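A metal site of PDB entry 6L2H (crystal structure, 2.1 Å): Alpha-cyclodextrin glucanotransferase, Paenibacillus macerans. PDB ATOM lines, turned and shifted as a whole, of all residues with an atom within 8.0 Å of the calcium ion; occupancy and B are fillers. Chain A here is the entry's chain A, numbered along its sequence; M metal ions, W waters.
Water W1 lies within hydrogen-bond range of the backbone carbonyl oxygen of Ile 200, the backbone carbonyl oxygen of Asn 139 and a ring nitrogen (ND1) of His 202.
The calcium ion is bound by OD1 of Asn 139 (2.3 Å), O of His 233 (2.4 Å), O of Ile 190 (2.5 Å), water W3 (2.5 Å), OD1 of Asp 199 (2.6 Å), OD2 of Asp 199 (2.6 Å), water W2 (2.7 Å) and water W1 (2.7 Å).
The calcium ion has eight donor atoms within binding distance.
The backbone carbonyl oxygen (O) of Asn 139 is in hydrogen-bond range of the backbone NH (N) of Ile 200 (3.0 Å).
A ring nitrogen (ND1) of His 233 is in hydrogen-bond range of the backbone carbonyl oxygen of Gly 189 (2.7 Å).
The backbone carbonyl oxygen (O) of Asp 199 is in hydrogen-bond range of the backbone NH (N) of His 176 (2.8 Å).
N of Asn 139 lies within hydrogen-bond range of SD of Met 234 (3.5 Å).
The side-chain amide nitrogen (ND2) of Asn 139 sits at hydrogen-bond distance from a ring nitrogen (ND1) of His 140, at 3.1 Å.
Four residues have an atom within 4 Å of the calcium ion: Asn 139, Ile 190, Asp 199 and His 233.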
ATOM      1  N   PRO A 138      14.183  10.989 -11.546  1.00  0.00           N
ATOM      2  CA  PRO A 138      15.070  11.849 -10.766  1.00  0.00           C
ATOM      3  C   PRO A 138      14.925  13.344 -11.073  1.00  0.00           C
ATOM      4  O   PRO A 138      15.661  14.147 -10.503  1.00  0.00           O
ATOM      5  CB  PRO A 138      16.461  11.350 -11.167  1.00  0.00           C
ATOM      6  CG  PRO A 138      16.279  10.939 -12.604  1.00  0.00           C
ATOM      7  CD  PRO A 138      14.867  10.388 -12.703  1.00  0.00           C
ATOM      8  N   ASN A 139      13.993  13.722 -11.943  1.00  0.00           N
ATOM      9  CA  ASN A 139      13.794  15.138 -12.217  1.00  0.00           C
ATOM     10  C   ASN A 139      13.197  15.892 -11.024  1.00  0.00           C
ATOM     11  O   ASN A 139      13.463  17.080 -10.845  1.00  0.00           O
ATOM     12  CB  ASN A 139      12.890  15.356 -13.442  1.00  0.00           C
ATOM     13  CG  ASN A 139      12.596  16.828 -13.690  1.00  0.00           C
ATOM     14  OD1 ASN A 139      13.494  17.595 -14.044  1.00  0.00           O
ATOM     15  ND2 ASN A 139      11.349  17.238 -13.480  1.00  0.00           N
ATOM     16  N   HIS A 140      12.393  15.207 -10.223  1.00  0.00           N
ATOM     17  CA  HIS A 140      11.586  15.892  -9.230  1.00  0.00           C
ATOM     18  C   HIS A 140      11.142  14.985  -8.085  1.00  0.00           C
ATOM     19  O   HIS A 140      11.324  13.771  -8.136  1.00  0.00           O
ATOM     20  CB  HIS A 140      10.338  16.478  -9.900  1.00  0.00           C
ATOM     21  CG  HIS A 140       9.501  15.448 -10.594  1.00  0.00           C
ATOM     22  ND1 HIS A 140       9.546  15.251 -11.961  1.00  0.00           N
ATOM     23  CD2 HIS A 140       8.625  14.545 -10.111  1.00  0.00           C
ATOM     24  CE1 HIS A 140       8.726  14.279 -12.288  1.00  0.00           C
ATOM     25  NE2 HIS A 140       8.144  13.834 -11.187  1.00  0.00           N
ATOM     26  N   HIS A 176      15.483  23.673  -7.366  1.00  0.00           N
ATOM     27  CA  HIS A 176      15.482  24.942  -8.072  1.00  0.00           C
ATOM     28  C   HIS A 176      14.381  25.826  -7.508  1.00  0.00           C
ATOM     29  O   HIS A 176      13.399  25.331  -6.956  1.00  0.00           O
ATOM     30  CB  HIS A 176      15.266  24.719  -9.578  1.00  0.00           C
ATOM     31  CG  HIS A 176      16.413  24.033 -10.250  1.00  0.00           C
ATOM     32  ND1 HIS A 176      16.244  22.910 -11.038  1.00  0.00           N
ATOM     33  CD2 HIS A 176      17.737  24.300 -10.262  1.00  0.00           C
ATOM     34  CE1 HIS A 176      17.413  22.524 -11.502  1.00  0.00           C
ATOM     35  NE2 HIS A 176      18.340  23.348 -11.050  1.00  0.00           N
ATOM     36  N   ILE A 186      13.389  24.532 -24.279  1.00  0.00           N
ATOM     37  CA  ILE A 186      13.970  23.415 -23.547  1.00  0.00           C
ATOM     38  C   ILE A 186      14.638  23.900 -22.255  1.00  0.00           C
ATOM     39  O   ILE A 186      14.463  23.290 -21.196  1.00  0.00           O
ATOM     40  CB  ILE A 186      14.972  22.646 -24.412  1.00  0.00           C
ATOM     41  CG1 ILE A 186      14.242  22.030 -25.610  1.00  0.00           C
ATOM     42  CG2 ILE A 186      15.676  21.576 -23.592  1.00  0.00           C
ATOM     43  CD1 ILE A 186      15.102  21.120 -26.435  1.00  0.00           C
ATOM     44  N   GLU A 187      15.377  24.998 -22.343  1.00  0.00           N
ATOM     45  CA  GLU A 187      16.001  25.579 -21.143  1.00  0.00           C
ATOM     46  C   GLU A 187      14.961  25.858 -20.072  1.00  0.00           C
ATOM     47  O   GLU A 187      15.144  25.520 -18.917  1.00  0.00           O
ATOM     48  CB  GLU A 187      16.743  26.881 -21.465  1.00  0.00           C
ATOM     49  CG  GLU A 187      17.239  27.573 -20.191  1.00  0.00           C
ATOM     50  CD  GLU A 187      17.727  28.995 -20.404  1.00  0.00           C
ATOM     51  OE1 GLU A 187      17.435  29.580 -21.459  1.00  0.00           O
ATOM     52  OE2 GLU A 187      18.391  29.539 -19.481  1.00  0.00           O
ATOM     53  N   ASP A 188      13.874  26.504 -20.481  1.00  0.00           N
ATOM     54  CA  ASP A 188      12.814  26.865 -19.548  1.00  0.00           C
ATOM     55  C   ASP A 188      12.236  25.609 -18.881  1.00  0.00           C
ATOM     56  O   ASP A 188      11.983  25.598 -17.677  1.00  0.00           O
ATOM     57  CB  ASP A 188      11.715  27.653 -20.271  1.00  0.00           C
ATOM     58  CG  ASP A 188      10.773  28.342 -19.305  1.00  0.00           C
ATOM     59  OD1 ASP A 188       9.840  27.680 -18.810  1.00  0.00           O
ATOM     60  OD2 ASP A 188      10.972  29.553 -19.042  1.00  0.00           O
ATOM     61  N   GLY A 189      12.061  24.557 -19.674  1.00  0.00           N
ATOM     62  CA  GLY A 189      11.516  23.295 -19.177  1.00  0.00           C
ATOM     63  C   GLY A 189      12.484  22.456 -18.349  1.00  0.00           C
ATOM     64  O   GLY A 189      12.071  21.501 -17.682  1.00  0.00           O
ATOM     65  N   ILE A 190      13.769  22.802 -18.389  1.00  0.00           N
ATOM     66  CA  ILE A 190      14.774  22.065 -17.619  1.00  0.00           C
ATOM     67  C   ILE A 190      14.981  22.632 -16.211  1.00  0.00           C
ATOM     68  O   ILE A 190      15.000  21.897 -15.221  1.00  0.00           O
ATOM     69  CB  ILE A 190      16.126  22.034 -18.348  1.00  0.00           C
ATOM     70  CG1 ILE A 190      16.035  21.151 -19.587  1.00  0.00           C
ATOM     71  CG2 ILE A 190      17.244  21.518 -17.443  1.00  0.00           C
ATOM     72  CD1 ILE A 190      17.350  21.014 -20.328  1.00  0.00           C
ATOM     73  N   TYR A 191      15.133  23.953 -16.124  1.00  0.00           N
ATOM     74  CA  TYR A 191      15.535  24.566 -14.869  1.00  0.00           C
ATOM     75  C   TYR A 191      14.384  25.227 -14.111  1.00  0.00           C
ATOM     76  O   TYR A 191      14.569  25.755 -13.023  1.00  0.00           O
ATOM     77  CB  TYR A 191      16.652  25.582 -15.129  1.00  0.00           C
ATOM     78  CG  TYR A 191      17.880  24.900 -15.675  1.00  0.00           C
ATOM     79  CD1 TYR A 191      18.664  24.100 -14.852  1.00  0.00           C
ATOM     80  CD2 TYR A 191      18.250  25.027 -17.009  1.00  0.00           C
ATOM     81  CE1 TYR A 191      19.781  23.454 -15.350  1.00  0.00           C
ATOM     82  CE2 TYR A 191      19.374  24.393 -17.508  1.00  0.00           C
ATOM     83  CZ  TYR A 191      20.133  23.610 -16.679  1.00  0.00           C
ATOM     84  OH  TYR A 191      21.240  22.963 -17.167  1.00  0.00           O
ATOM     85  N   LYS A 192      13.184  25.173 -14.685  1.00  0.00           N
ATOM     86  CA  LYS A 192      11.986  25.554 -13.956  1.00  0.00           C
ATOM     87  C   LYS A 192      11.184  24.288 -13.644  1.00  0.00           C
ATOM     88  O   LYS A 192      11.498  23.210 -14.155  1.00  0.00           O
ATOM     89  CB  LYS A 192      11.162  26.568 -14.762  1.00  0.00           C
ATOM     90  CG  LYS A 192      11.859  27.928 -14.903  1.00  0.00           C
ATOM     91  CD  LYS A 192      11.017  28.934 -15.677  1.00  0.00           C
ATOM     92  CE  LYS A 192      11.779  30.237 -15.916  1.00  0.00           C
ATOM     93  NZ  LYS A 192      10.892  31.259 -16.553  1.00  0.00           N
ATOM     94  N   ASN A 193      10.169  24.414 -12.786  1.00  0.00           N
ATOM     95  CA  ASN A 193       9.405  23.250 -12.329  1.00  0.00           C
ATOM     96  C   ASN A 193       8.528  22.652 -13.425  1.00  0.00           C
ATOM     97  O   ASN A 193       7.916  23.375 -14.205  1.00  0.00           O
ATOM     98  CB  ASN A 193       8.517  23.623 -11.126  1.00  0.00           C
ATOM     99  CG  ASN A 193       9.308  24.241  -9.987  1.00  0.00           C
ATOM    100  OD1 ASN A 193      10.520  24.064  -9.888  1.00  0.00           O
ATOM    101  ND2 ASN A 193       8.611  24.978  -9.122  1.00  0.00           N
ATOM    102  N   LEU A 194       8.481  21.319 -13.484  1.00  0.00           N
ATOM    103  CA  LEU A 194       7.455  20.610 -14.239  1.00  0.00           C
ATOM    104  C   LEU A 194       6.087  20.665 -13.577  1.00  0.00           C
ATOM    105  O   LEU A 194       5.828  19.890 -12.663  1.00  0.00           O
ATOM    106  CB  LEU A 194       7.802  19.132 -14.384  1.00  0.00           C
ATOM    107  CG  LEU A 194       8.058  18.475 -15.734  1.00  0.00           C
ATOM    108  CD1 LEU A 194       7.951  16.961 -15.587  1.00  0.00           C
ATOM    109  CD2 LEU A 194       7.103  18.995 -16.806  1.00  0.00           C
ATOM    110  N   LEU A 197       5.841  20.456  -9.611  1.00  0.00           N
ATOM    111  CA  LEU A 197       6.742  19.463  -9.051  1.00  0.00           C
ATOM    112  C   LEU A 197       8.052  20.098  -8.626  1.00  0.00           C
ATOM    113  O   LEU A 197       8.725  20.730  -9.433  1.00  0.00           O
ATOM    114  CB  LEU A 197       6.984  18.340 -10.056  1.00  0.00           C
ATOM    115  CG  LEU A 197       5.718  17.608 -10.490  1.00  0.00           C
ATOM    116  CD1 LEU A 197       6.002  16.654 -11.638  1.00  0.00           C
ATOM    117  CD2 LEU A 197       5.080  16.871  -9.315  1.00  0.00           C
ATOM    118  N   ALA A 198       8.391  19.926  -7.354  1.00  0.00           N
ATOM    119  CA  ALA A 198       9.650  20.426  -6.813  1.00  0.00           C
ATOM    120  C   ALA A 198      10.805  19.880  -7.634  1.00  0.00           C
ATOM    121  O   ALA A 198      11.010  18.657  -7.703  1.00  0.00           O
ATOM    122  CB  ALA A 198       9.792  20.046  -5.356  1.00  0.00           C
ATOM    123  N   ASP A 199      11.559  20.778  -8.254  1.00  0.00           N
ATOM    124  CA  ASP A 199      12.552  20.399  -9.247  1.00  0.00           C
ATOM    125  C   ASP A 199      13.950  20.177  -8.662  1.00  0.00           C
ATOM    126  O   ASP A 199      14.555  21.101  -8.121  1.00  0.00           O
ATOM    127  CB  ASP A 199      12.625  21.484 -10.322  1.00  0.00           C
ATOM    128  CG  ASP A 199      13.178  20.962 -11.613  1.00  0.00           C
ATOM    129  OD1 ASP A 199      12.615  19.990 -12.133  1.00  0.00           O
ATOM    130  OD2 ASP A 199      14.187  21.519 -12.094  1.00  0.00           O
ATOM    131  N   ILE A 200      14.453  18.950  -8.788  1.00  0.00           N
ATOM    132  CA  ILE A 200      15.780  18.596  -8.252  1.00  0.00           C
ATOM    133  C   ILE A 200      16.913  19.412  -8.890  1.00  0.00           C
ATOM    134  O   ILE A 200      16.993  19.548 -10.106  1.00  0.00           O
ATOM    135  CB  ILE A 200      16.080  17.095  -8.457  1.00  0.00           C
ATOM    136  CG1 ILE A 200      15.062  16.228  -7.691  1.00  0.00           C
ATOM    137  CG2 ILE A 200      17.493  16.766  -8.003  1.00  0.00           C
ATOM    138  CD1 ILE A 200      15.179  16.347  -6.170  1.00  0.00           C
ATOM    139  N   ASN A 201      17.784  19.948  -8.038  1.00  0.00           N
ATOM    140  CA  ASN A 201      19.001  20.627  -8.472  1.00  0.00           C
ATOM    141  C   ASN A 201      20.142  19.616  -8.581  1.00  0.00           C
ATOM    142  O   ASN A 201      20.767  19.274  -7.589  1.00  0.00           O
ATOM    143  CB  ASN A 201      19.356  21.741  -7.479  1.00  0.00           C
ATOM    144  CG  ASN A 201      20.686  22.418  -7.796  1.00  0.00           C
ATOM    145  OD1 ASN A 201      21.234  22.269  -8.895  1.00  0.00           O
ATOM    146  ND2 ASN A 201      21.222  23.160  -6.835  1.00  0.00           N
ATOM    147  N   HIS A 202      20.425  19.151  -9.793  1.00  0.00           N
ATOM    148  CA  HIS A 202      21.455  18.130  -9.977  1.00  0.00           C
ATOM    149  C   HIS A 202      22.856  18.724 -10.009  1.00  0.00           C
ATOM    150  O   HIS A 202      23.840  17.990 -10.067  1.00  0.00           O
ATOM    151  CB  HIS A 202      21.205  17.308 -11.245  1.00  0.00           C
ATOM    152  CG  HIS A 202      19.858  16.658 -11.292  1.00  0.00           C
ATOM    153  ND1 HIS A 202      18.766  17.238 -11.912  1.00  0.00           N
ATOM    154  CD2 HIS A 202      19.415  15.484 -10.788  1.00  0.00           C
ATOM    155  CE1 HIS A 202      17.721  16.440 -11.794  1.00  0.00           C
ATOM    156  NE2 HIS A 202      18.086  15.367 -11.110  1.00  0.00           N
ATOM    157  N   ALA A 230      10.760  12.120 -17.793  1.00  0.00           N
ATOM    158  CA  ALA A 230      11.022  13.541 -18.058  1.00  0.00           C
ATOM    159  C   ALA A 230      12.470  13.845 -18.439  1.00  0.00           C
ATOM    160  O   ALA A 230      13.072  14.786 -17.912  1.00  0.00           O
ATOM    161  CB  ALA A 230      10.611  14.375 -16.841  1.00  0.00           C
ATOM    162  N   LYS A 232      13.508  15.282 -20.997  1.00  0.00           N
ATOM    163  CA  LYS A 232      13.555  16.569 -21.673  1.00  0.00           C
ATOM    164  C   LYS A 232      13.704  17.685 -20.639  1.00  0.00           C
ATOM    165  O   LYS A 232      14.045  18.815 -20.987  1.00  0.00           O
ATOM    166  CB  LYS A 232      12.292  16.781 -22.515  1.00  0.00           C
ATOM    167  CG  LYS A 232      12.320  17.972 -23.480  1.00  0.00           C
ATOM    168  CD  LYS A 232      10.998  18.045 -24.267  1.00  0.00           C
ATOM    169  CE  LYS A 232      10.949  19.258 -25.189  1.00  0.00           C
ATOM    170  NZ  LYS A 232       9.635  19.341 -25.886  1.00  0.00           N
ATOM    171  N   HIS A 233      13.453  17.360 -19.384  1.00  0.00           N
ATOM    172  CA  HIS A 233      13.384  18.358 -18.317  1.00  0.00           C
ATOM    173  C   HIS A 233      14.554  18.274 -17.361  1.00  0.00           C
ATOM    174  O   HIS A 233      14.573  18.943 -16.317  1.00  0.00           O
ATOM    175  CB  HIS A 233      12.049  18.226 -17.587  1.00  0.00           C
ATOM    176  CG  HIS A 233      10.877  18.447 -18.488  1.00  0.00           C
ATOM    177  ND1 HIS A 233      10.510  19.705 -18.932  1.00  0.00           N
ATOM    178  CD2 HIS A 233      10.022  17.580 -19.081  1.00  0.00           C
ATOM    179  CE1 HIS A 233       9.476  19.599 -19.743  1.00  0.00           C
ATOM    180  NE2 HIS A 233       9.159  18.321 -19.845  1.00  0.00           N
ATOM    181  N   MET A 234      15.539  17.448 -17.717  1.00  0.00           N
ATOM    182  CA  MET A 234      16.825  17.399 -17.028  1.00  0.00           C
ATOM    183  C   MET A 234      17.940  17.719 -18.019  1.00  0.00           C
ATOM    184  O   MET A 234      17.769  17.528 -19.213  1.00  0.00           O
ATOM    185  CB  MET A 234      17.046  16.020 -16.393  1.00  0.00           C
ATOM    186  CG  MET A 234      16.070  15.718 -15.266  1.00  0.00           C
ATOM    187  SD  MET A 234      16.244  14.058 -14.569  1.00  0.00           S
ATOM    188  CE  MET A 234      15.643  13.027 -15.894  1.00  0.00           C
ATOM    189  N   PRO A 235      19.071  18.242 -17.529  1.00  0.00           N
ATOM    190  CA  PRO A 235      20.177  18.559 -18.428  1.00  0.00           C
ATOM    191  C   PRO A 235      20.676  17.306 -19.131  1.00  0.00           C
ATOM    192  O   PRO A 235      20.789  16.257 -18.504  1.00  0.00           O
ATOM    193  CB  PRO A 235      21.258  19.120 -17.489  1.00  0.00           C
ATOM    194  CG  PRO A 235      20.516  19.572 -16.275  1.00  0.00           C
ATOM    195  CD  PRO A 235      19.376  18.611 -16.129  1.00  0.00           C
HETATM  196 CA    CA M   1      14.305  19.785 -14.046  1.00  0.00          CA
HETATM  197  O   HOH W   1      15.544  18.540 -12.035  1.00  0.00           O
HETATM  198  O   HOH W   2      12.054  20.577 -15.219  1.00  0.00           O
HETATM  199  O   HOH W   3      16.825  19.946 -14.158  1.00  0.00           O
